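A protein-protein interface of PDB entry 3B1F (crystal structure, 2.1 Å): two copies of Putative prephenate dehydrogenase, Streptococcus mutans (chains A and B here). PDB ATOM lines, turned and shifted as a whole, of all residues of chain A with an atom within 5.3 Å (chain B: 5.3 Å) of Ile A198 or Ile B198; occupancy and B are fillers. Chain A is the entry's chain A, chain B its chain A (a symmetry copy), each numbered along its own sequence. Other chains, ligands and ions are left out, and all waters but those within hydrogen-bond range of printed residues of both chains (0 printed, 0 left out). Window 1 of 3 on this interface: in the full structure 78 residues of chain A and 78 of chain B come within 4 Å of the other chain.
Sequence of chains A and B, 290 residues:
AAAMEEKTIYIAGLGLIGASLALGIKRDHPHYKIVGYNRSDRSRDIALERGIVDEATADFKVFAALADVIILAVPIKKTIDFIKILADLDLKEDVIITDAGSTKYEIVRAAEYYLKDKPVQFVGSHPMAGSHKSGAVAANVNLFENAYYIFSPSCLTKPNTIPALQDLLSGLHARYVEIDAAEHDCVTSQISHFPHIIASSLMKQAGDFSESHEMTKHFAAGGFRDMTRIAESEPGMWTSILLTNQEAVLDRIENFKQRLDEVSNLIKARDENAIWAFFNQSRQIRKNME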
ATOM      1  N   PHE A 194     -31.437  11.939 -24.843  1.00  0.00           N
ATOM      2  CA  PHE A 194     -30.654  12.657 -23.833  1.00  0.00           C
ATOM      3  C   PHE A 194     -29.630  11.645 -23.230  1.00  0.00           C
ATOM      4  O   PHE A 194     -28.469  11.991 -23.080  1.00  0.00           O
ATOM      5  CB  PHE A 194     -31.557  13.326 -22.739  1.00  0.00           C
ATOM      6  CG  PHE A 194     -30.762  13.967 -21.591  1.00  0.00           C
ATOM      7  CD1 PHE A 194     -29.782  14.934 -21.840  1.00  0.00           C
ATOM      8  CD2 PHE A 194     -30.934  13.532 -20.289  1.00  0.00           C
ATOM      9  CE1 PHE A 194     -29.021  15.494 -20.816  1.00  0.00           C
ATOM     10  CE2 PHE A 194     -30.180  14.091 -19.265  1.00  0.00           C
ATOM     11  CZ  PHE A 194     -29.191  15.040 -19.532  1.00  0.00           C
ATOM     12  N   PRO A 195     -30.041  10.390 -22.941  1.00  0.00           N
ATOM     13  CA  PRO A 195     -28.949   9.502 -22.567  1.00  0.00           C
ATOM     14  C   PRO A 195     -27.795   9.449 -23.575  1.00  0.00           C
ATOM     15  O   PRO A 195     -26.643   9.309 -23.146  1.00  0.00           O
ATOM     16  CB  PRO A 195     -29.630   8.110 -22.486  1.00  0.00           C
ATOM     17  CG  PRO A 195     -31.090   8.455 -22.108  1.00  0.00           C
ATOM     18  CD  PRO A 195     -31.395   9.785 -22.676  1.00  0.00           C
ATOM     19  N   HIS A 196     -28.072   9.550 -24.885  1.00  0.00           N
ATOM     20  CA  HIS A 196     -26.969   9.501 -25.855  1.00  0.00           C
ATOM     21  C   HIS A 196     -26.042  10.742 -25.697  1.00  0.00           C
ATOM     22  O   HIS A 196     -24.777  10.659 -25.822  1.00  0.00           O
ATOM     23  CB  HIS A 196     -27.498   9.281 -27.306  1.00  0.00           C
ATOM     24  CG  HIS A 196     -26.385   8.965 -28.280  1.00  0.00           C
ATOM     25  ND1 HIS A 196     -26.016   7.675 -28.618  1.00  0.00           N
ATOM     26  CD2 HIS A 196     -25.499   9.791 -28.922  1.00  0.00           C
ATOM     27  CE1 HIS A 196     -24.949   7.737 -29.425  1.00  0.00           C
ATOM     28  NE2 HIS A 196     -24.628   9.007 -29.639  1.00  0.00           N
ATOM     29  N   ILE A 197     -26.659  11.901 -25.441  1.00  0.00           N
ATOM     30  CA  ILE A 197     -25.923  13.134 -25.151  1.00  0.00           C
ATOM     31  C   ILE A 197     -25.052  12.931 -23.947  1.00  0.00           C
ATOM     32  O   ILE A 197     -23.862  13.279 -23.928  1.00  0.00           O
ATOM     33  CB  ILE A 197     -26.913  14.303 -24.884  1.00  0.00           C
ATOM     34  CG1 ILE A 197     -27.547  14.684 -26.226  1.00  0.00           C
ATOM     35  CG2 ILE A 197     -26.187  15.592 -24.336  1.00  0.00           C
ATOM     36  CD1 ILE A 197     -28.523  15.789 -26.190  1.00  0.00           C
ATOM     37  N   ILE A 198     -25.625  12.311 -22.924  1.00  0.00           N
ATOM     38  CA  ILE A 198     -24.823  12.144 -21.761  1.00  0.00           C
ATOM     39  C   ILE A 198     -23.655  11.196 -21.988  1.00  0.00           C
ATOM     40  O   ILE A 198     -22.589  11.414 -21.464  1.00  0.00           O
ATOM     41  CB  ILE A 198     -25.657  11.482 -20.653  1.00  0.00           C
ATOM     42  CG1 ILE A 198     -26.509  12.544 -20.033  1.00  0.00           C
ATOM     43  CG2 ILE A 198     -24.691  10.847 -19.639  1.00  0.00           C
ATOM     44  CD1 ILE A 198     -27.620  11.756 -19.128  1.00  0.00           C
ATOM     45  N   ALA A 199     -23.910  10.072 -22.632  1.00  0.00           N
ATOM     46  CA  ALA A 199     -22.867   9.105 -22.925  1.00  0.00           C
ATOM     47  C   ALA A 199     -21.773   9.756 -23.775  1.00  0.00           C
ATOM     48  O   ALA A 199     -20.569   9.532 -23.540  1.00  0.00           O
ATOM     49  CB  ALA A 199     -23.439   7.838 -23.659  1.00  0.00           C
ATOM     50  N   SER A 200     -22.165  10.591 -24.721  1.00  0.00           N
ATOM     51  CA  SER A 200     -21.127  11.224 -25.596  1.00  0.00           C
ATOM     52  C   SER A 200     -20.273  12.280 -24.851  1.00  0.00           C
ATOM     53  O   SER A 200     -19.074  12.370 -25.061  1.00  0.00           O
ATOM     54  CB  SER A 200     -21.842  11.874 -26.769  1.00  0.00           C
ATOM     55  OG  SER A 200     -22.447  10.842 -27.551  1.00  0.00           O
ATOM     56  N   SER A 201     -20.932  13.085 -24.007  1.00  0.00           N
ATOM     57  CA  SER A 201     -20.303  14.089 -23.120  1.00  0.00           C
ATOM     58  C   SER A 201     -19.365  13.449 -22.103  1.00  0.00           C
ATOM     59  O   SER A 201     -18.245  13.930 -21.898  1.00  0.00           O
ATOM     60  CB  SER A 201     -21.369  14.843 -22.322  1.00  0.00           C
ATOM     61  OG  SER A 201     -22.192  15.565 -23.189  1.00  0.00           O
ATOM     62  N   LEU A 202     -19.840  12.374 -21.458  1.00  0.00           N
ATOM     63  CA  LEU A 202     -19.013  11.633 -20.541  1.00  0.00           C
ATOM     64  C   LEU A 202     -17.738  11.039 -21.233  1.00  0.00           C
ATOM     65  O   LEU A 202     -16.653  11.098 -20.678  1.00  0.00           O
ATOM     66  CB  LEU A 202     -19.802  10.501 -19.923  1.00  0.00           C
ATOM     67  CG  LEU A 202     -19.019   9.669 -18.877  1.00  0.00           C
ATOM     68  CD1 LEU A 202     -18.274  10.582 -17.760  1.00  0.00           C
ATOM     69  CD2 LEU A 202     -19.961   8.541 -18.262  1.00  0.00           C
ATOM     70  N   MET A 203     -17.887  10.445 -22.405  1.00  0.00           N
ATOM     71  CA  MET A 203     -16.702   9.864 -23.137  1.00  0.00           C
ATOM     72  C   MET A 203     -15.662  10.965 -23.449  1.00  0.00           C
ATOM     73  O   MET A 203     -14.433  10.788 -23.324  1.00  0.00           O
ATOM     74  CB  MET A 203     -17.186   9.217 -24.446  1.00  0.00           C
ATOM     75  CG  MET A 203     -16.140   8.451 -25.278  1.00  0.00           C
ATOM     76  SD  MET A 203     -15.250   7.060 -24.187  1.00  0.00           S
ATOM     77  CE  MET A 203     -16.186   5.493 -24.760  1.00  0.00           C
ATOM     78  N   MET A 227     -21.642   2.807 -19.688  1.00  0.00           N
ATOM     79  CA  MET A 227     -22.302   4.085 -19.876  1.00  0.00           C
ATOM     80  C   MET A 227     -21.773   4.829 -21.049  1.00  0.00           C
ATOM     81  O   MET A 227     -22.122   6.009 -21.262  1.00  0.00           O
ATOM     82  CB  MET A 227     -22.122   4.931 -18.651  1.00  0.00           C
ATOM     83  CG  MET A 227     -22.241   4.033 -17.514  1.00  0.00           C
ATOM     84  SD  MET A 227     -22.460   5.313 -16.163  1.00  0.00           S
ATOM     85  CE  MET A 227     -24.075   6.259 -16.854  1.00  0.00           C
ATOM     86  N   PHE A 256     -31.492  18.100 -15.902  1.00  0.00           N
ATOM     87  CA  PHE A 256     -30.339  17.367 -15.437  1.00  0.00           C
ATOM     88  C   PHE A 256     -29.274  18.261 -14.762  1.00  0.00           C
ATOM     89  O   PHE A 256     -28.623  17.843 -13.821  1.00  0.00           O
ATOM     90  CB  PHE A 256     -29.703  16.596 -16.580  1.00  0.00           C
ATOM     91  CG  PHE A 256     -28.886  15.468 -16.126  1.00  0.00           C
ATOM     92  CD1 PHE A 256     -29.489  14.283 -15.699  1.00  0.00           C
ATOM     93  CD2 PHE A 256     -27.466  15.571 -16.153  1.00  0.00           C
ATOM     94  CE1 PHE A 256     -28.684  13.188 -15.260  1.00  0.00           C
ATOM     95  CE2 PHE A 256     -26.701  14.528 -15.728  1.00  0.00           C
ATOM     96  CZ  PHE A 256     -27.288  13.314 -15.301  1.00  0.00           C
ATOM     97  N   LEU A 260     -27.877  17.927 -10.970  1.00  0.00           N
ATOM     98  CA  LEU A 260     -26.462  17.880 -10.602  1.00  0.00           C
ATOM     99  C   LEU A 260     -26.126  18.936  -9.483  1.00  0.00           C
ATOM    100  O   LEU A 260     -25.260  18.661  -8.586  1.00  0.00           O
ATOM    101  CB  LEU A 260     -25.531  18.097 -11.849  1.00  0.00           C
ATOM    102  CG  LEU A 260     -25.458  17.006 -12.958  1.00  0.00           C
ATOM    103  CD1 LEU A 260     -24.552  17.422 -14.201  1.00  0.00           C
ATOM    104  CD2 LEU A 260     -24.929  15.686 -12.374  1.00  0.00           C
ATOM    105  N   PHE B 194     -18.014   9.625 -10.464  1.00  0.00           N
ATOM    106  CA  PHE B 194     -18.889  10.605 -11.115  1.00  0.00           C
ATOM    107  C   PHE B 194     -19.816   9.822 -12.096  1.00  0.00           C
ATOM    108  O   PHE B 194     -21.009  10.078 -12.120  1.00  0.00           O
ATOM    109  CB  PHE B 194     -18.083  11.747 -11.826  1.00  0.00           C
ATOM    110  CG  PHE B 194     -18.965  12.711 -12.635  1.00  0.00           C
ATOM    111  CD1 PHE B 194     -20.033  13.389 -12.038  1.00  0.00           C
ATOM    112  CD2 PHE B 194     -18.777  12.858 -13.998  1.00  0.00           C
ATOM    113  CE1 PHE B 194     -20.869  14.233 -12.767  1.00  0.00           C
ATOM    114  CE2 PHE B 194     -19.607  13.702 -14.726  1.00  0.00           C
ATOM    115  CZ  PHE B 194     -20.682  14.356 -14.120  1.00  0.00           C
ATOM    116  N   PRO B 195     -19.285   8.840 -12.858  1.00  0.00           N
ATOM    117  CA  PRO B 195     -20.288   8.071 -13.582  1.00  0.00           C
ATOM    118  C   PRO B 195     -21.408   7.497 -12.706  1.00  0.00           C
ATOM    119  O   PRO B 195     -22.548   7.425 -13.181  1.00  0.00           O
ATOM    120  CB  PRO B 195     -19.469   6.908 -14.203  1.00  0.00           C
ATOM    121  CG  PRO B 195     -18.060   7.524 -14.378  1.00  0.00           C
ATOM    122  CD  PRO B 195     -17.882   8.535 -13.315  1.00  0.00           C
ATOM    123  N   HIS B 196     -21.114   7.089 -11.461  1.00  0.00           N
ATOM    124  CA  HIS B 196     -22.185   6.540 -10.617  1.00  0.00           C
ATOM    125  C   HIS B 196     -23.238   7.638 -10.282  1.00  0.00           C
ATOM    126  O   HIS B 196     -24.485   7.382 -10.229  1.00  0.00           O
ATOM    127  CB  HIS B 196     -21.605   5.810  -9.368  1.00  0.00           C
ATOM    128  CG  HIS B 196     -22.658   5.015  -8.627  1.00  0.00           C
ATOM    129  ND1 HIS B 196     -22.885   3.668  -8.846  1.00  0.00           N
ATOM    130  CD2 HIS B 196     -23.610   5.416  -7.727  1.00  0.00           C
ATOM    131  CE1 HIS B 196     -23.935   3.290  -8.107  1.00  0.00           C
ATOM    132  NE2 HIS B 196     -24.380   4.325  -7.405  1.00  0.00           N
ATOM    133  N   ILE B 197     -22.749   8.858 -10.035  1.00  0.00           N
ATOM    134  CA  ILE B 197     -23.613  10.020  -9.819  1.00  0.00           C
ATOM    135  C   ILE B 197     -24.485  10.232 -11.022  1.00  0.00           C
ATOM    136  O   ILE B 197     -25.705  10.434 -10.924  1.00  0.00           O
ATOM    137  CB  ILE B 197     -22.756  11.294  -9.571  1.00  0.00           C
ATOM    138  CG1 ILE B 197     -22.135  11.163  -8.176  1.00  0.00           C
ATOM    139  CG2 ILE B 197     -23.621  12.612  -9.568  1.00  0.00           C
ATOM    140  CD1 ILE B 197     -21.279  12.282  -7.742  1.00  0.00           C
ATOM    141  N   ILE B 198     -23.874  10.140 -12.195  1.00  0.00           N
ATOM    142  CA  ILE B 198     -24.679  10.374 -13.344  1.00  0.00           C
ATOM    143  C   ILE B 198     -25.739   9.301 -13.543  1.00  0.00           C
ATOM    144  O   ILE B 198     -26.832   9.601 -13.958  1.00  0.00           O
ATOM    145  CB  ILE B 198     -23.806  10.305 -14.606  1.00  0.00           C
ATOM    146  CG1 ILE B 198     -23.082  11.607 -14.727  1.00  0.00           C
ATOM    147  CG2 ILE B 198     -24.723  10.037 -15.811  1.00  0.00           C
ATOM    148  CD1 ILE B 198     -21.916  11.371 -15.848  1.00  0.00           C
ATOM    149  N   ALA B 199     -25.356   8.045 -13.402  1.00  0.00           N
ATOM    150  CA  ALA B 199     -26.287   6.940 -13.547  1.00  0.00           C
ATOM    151  C   ALA B 199     -27.423   7.077 -12.530  1.00  0.00           C
ATOM    152  O   ALA B 199     -28.603   6.844 -12.862  1.00  0.00           O
ATOM    153  CB  ALA B 199     -25.572   5.551 -13.373  1.00  0.00           C
ATOM    154  N   SER B 200     -27.099   7.495 -11.320  1.00  0.00           N
ATOM    155  CA  SER B 200     -28.178   7.612 -10.287  1.00  0.00           C
ATOM    156  C   SER B 200     -29.151   8.784 -10.561  1.00  0.00           C
ATOM    157  O   SER B 200     -30.348   8.658 -10.358  1.00  0.00           O
ATOM    158  CB  SER B 200     -27.507   7.804  -8.936  1.00  0.00           C
ATOM    159  OG  SER B 200     -26.783   6.612  -8.623  1.00  0.00           O
ATOM    160  N   SER B 201     -28.597   9.925 -10.994  1.00  0.00           N
ATOM    161  CA  SER B 201     -29.345  11.130 -11.414  1.00  0.00           C
ATOM    162  C   SER B 201     -30.234  10.862 -12.623  1.00  0.00           C
ATOM    163  O   SER B 201     -31.401  11.267 -12.641  1.00  0.00           O
ATOM    164  CB  SER B 201     -28.380  12.247 -11.817  1.00  0.00           C
ATOM    165  OG  SER B 201     -27.617  12.639 -10.715  1.00  0.00           O
ATOM    166  N   LEU B 202     -29.665  10.194 -13.636  1.00  0.00           N
ATOM    167  CA  LEU B 202     -30.432   9.804 -14.792  1.00  0.00           C
ATOM    168  C   LEU B 202     -31.623   8.854 -14.426  1.00  0.00           C
ATOM    169  O   LEU B 202     -32.720   9.020 -14.933  1.00  0.00           O
ATOM    170  CB  LEU B 202     -29.544   9.105 -15.797  1.00  0.00           C
ATOM    171  CG  LEU B 202     -30.260   8.690 -17.106  1.00  0.00           C
ATOM    172  CD1 LEU B 202     -31.118   9.894 -17.776  1.00  0.00           C
ATOM    173  CD2 LEU B 202     -29.220   8.009 -18.103  1.00  0.00           C
ATOM    174  N   MET B 203     -31.389   7.857 -13.590  1.00  0.00           N
ATOM    175  CA  MET B 203     -32.491   6.912 -13.181  1.00  0.00           C
ATOM    176  C   MET B 203     -33.632   7.680 -12.474  1.00  0.00           C
ATOM    177  O   MET B 203     -34.839   7.444 -12.686  1.00  0.00           O
ATOM    178  CB  MET B 203     -31.916   5.845 -12.233  1.00  0.00           C
ATOM    179  CG  MET B 203     -32.859   4.706 -11.803  1.00  0.00           C
ATOM    180  SD  MET B 203     -33.624   3.789 -13.382  1.00  0.00           S
ATOM    181  CE  MET B 203     -32.520   2.230 -13.470  1.00  0.00           C
ATOM    182  N   MET B 227     -26.928   2.393 -19.074  1.00  0.00           N
ATOM    183  CA  MET B 227     -26.399   3.547 -18.372  1.00  0.00           C
ATOM    184  C   MET B 227     -26.976   3.696 -17.010  1.00  0.00           C
ATOM    185  O   MET B 227     -26.746   4.719 -16.333  1.00  0.00           O
ATOM    186  CB  MET B 227     -26.691   4.791 -19.156  1.00  0.00           C
ATOM    187  CG  MET B 227     -26.506   4.446 -20.556  1.00  0.00           C
ATOM    188  SD  MET B 227     -26.448   6.177 -21.271  1.00  0.00           S
ATOM    189  CE  MET B 227     -24.925   6.925 -20.222  1.00  0.00           C
ATOM    190  N   PHE B 256     -18.787  18.838 -16.158  1.00  0.00           N
ATOM    191  CA  PHE B 256     -19.868  18.241 -16.904  1.00  0.00           C
ATOM    192  C   PHE B 256     -21.034  19.216 -17.184  1.00  0.00           C
ATOM    193  O   PHE B 256     -21.659  19.149 -18.228  1.00  0.00           O
ATOM    194  CB  PHE B 256     -20.396  17.013 -16.183  1.00  0.00           C
ATOM    195  CG  PHE B 256     -21.103  16.087 -17.070  1.00  0.00           C
ATOM    196  CD1 PHE B 256     -20.391  15.243 -17.925  1.00  0.00           C
ATOM    197  CD2 PHE B 256     -22.526  16.023 -17.035  1.00  0.00           C
ATOM    198  CE1 PHE B 256     -21.088  14.342 -18.786  1.00  0.00           C
ATOM    199  CE2 PHE B 256     -23.188  15.167 -17.861  1.00  0.00           C
ATOM    200  CZ  PHE B 256     -22.488  14.296 -18.728  1.00  0.00           C
ATOM    201  N   LEU B 260     -22.471  20.298 -20.818  1.00  0.00           N
ATOM    202  CA  LEU B 260     -23.881  20.258 -21.204  1.00  0.00           C
ATOM    203  C   LEU B 260     -24.349  21.635 -21.809  1.00  0.00           C
ATOM    204  O   LEU B 260     -25.201  21.657 -22.760  1.00  0.00           O
ATOM    205  CB  LEU B 260     -24.803  19.856 -19.996  1.00  0.00           C
ATOM    206  CG  LEU B 260     -24.739  18.410 -19.423  1.00  0.00           C
ATOM    207  CD1 LEU B 260     -25.656  18.194 -18.138  1.00  0.00           C
ATOM    208  CD2 LEU B 260     -25.142  17.391 -20.501  1.00  0.00           C
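The side-chain sulfur of Met A227 sits close to the backbone carbonyl oxygen of Pro B195, 3.7 Å away.
O of Pro A195 sits close to SD of Met B227.
The backbone carbonyl oxygen (O) of Ile B197 sits at hydrogen-bond distance from the side-chain hydroxyl (OG) of Ser B201, 2.9 Å away.
The backbone carbonyl oxygen (O) of Ile A197 is in hydrogen-bond range of the side-chain hydroxyl (OG) of Ser A201, 2.9 Å away.
Among the printed residues, pairs that only touch across the chains: Ile A198 with Ile B198 (3.9 Å), Ile A198 with Met B227 (3.97 Å), Ile A198 with Phe B256 (3.98 Å), Ala A199 with Met B227 (3.9 Å), Ser A201 with Phe B256 (3.6 Å), Leu A202 with Phe B256 (3.5 Å), Met A227 with Ile B198 (3.97 Å), Met A227 with Ala B199 (3.9 Å), Met A227 with Met B227 (3.1 Å), Phe A256 with Ile B198 (3.97 Å), Phe A256 with Ser B201 (3.6 Å), Phe A256 with Leu B202 (3.5 Å), Phe A256 with Leu B260 (3.8 Å) and Leu A260 with Phe B256 (3.8 Å).
Of the printed residues of chain B, Ala A199 touches Met B227 (3.9 Å).
Of the printed residues of chain B, Leu A260 touches Phe B256 (3.8 Å).
Ile A197 touches none of the printed residues of chain B.
Printed residues of chain B that touch a printed residue of chain A: Pro B195, Ile B198, Ala B199, Ser B201, Leu B202, Met B227, Phe B256 and Leu B260.
Hydrophobic or aromatic side chains of chain B within 4 Å of the printed part of chain A: Pro B195, Ile B198, Ala B199, Met B227, Phe B256 and Leu B260.
Printed residues of chain A that touch a printed residue of chain B: Pro A195, Ile A198, Ala A199, Ser A201, Leu A202, Met A227, Phe A256 and Leu A260.
Hydrophobic or aromatic side chains of chain A that line the printed part of chain B: Pro A195, Ile A198, Ala A199, Met A227, Phe A256 and Leu A260.
Along chain A the printed residues that touch a printed residue of chain B span positions 195 to 260.
Among the printed residues, 16 pairs touch across the chains.
Ile A198 touches its own counterpart, Ile B198.
Ile A198 touches Met B227, and with the chains exchanged Met A227 touches Ile B198.
Ile A198 touches Phe B256, and with the chains exchanged Phe A256 touches Ile B198.
Ser A201 touches Phe B256, and with the chains exchanged Phe A256 touches Ser B201.
13 positions are printed for both chains.
Of the 16 pairs that touch across the chains among the printed residues, 16 have their exchanged pair printed and touching as well.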
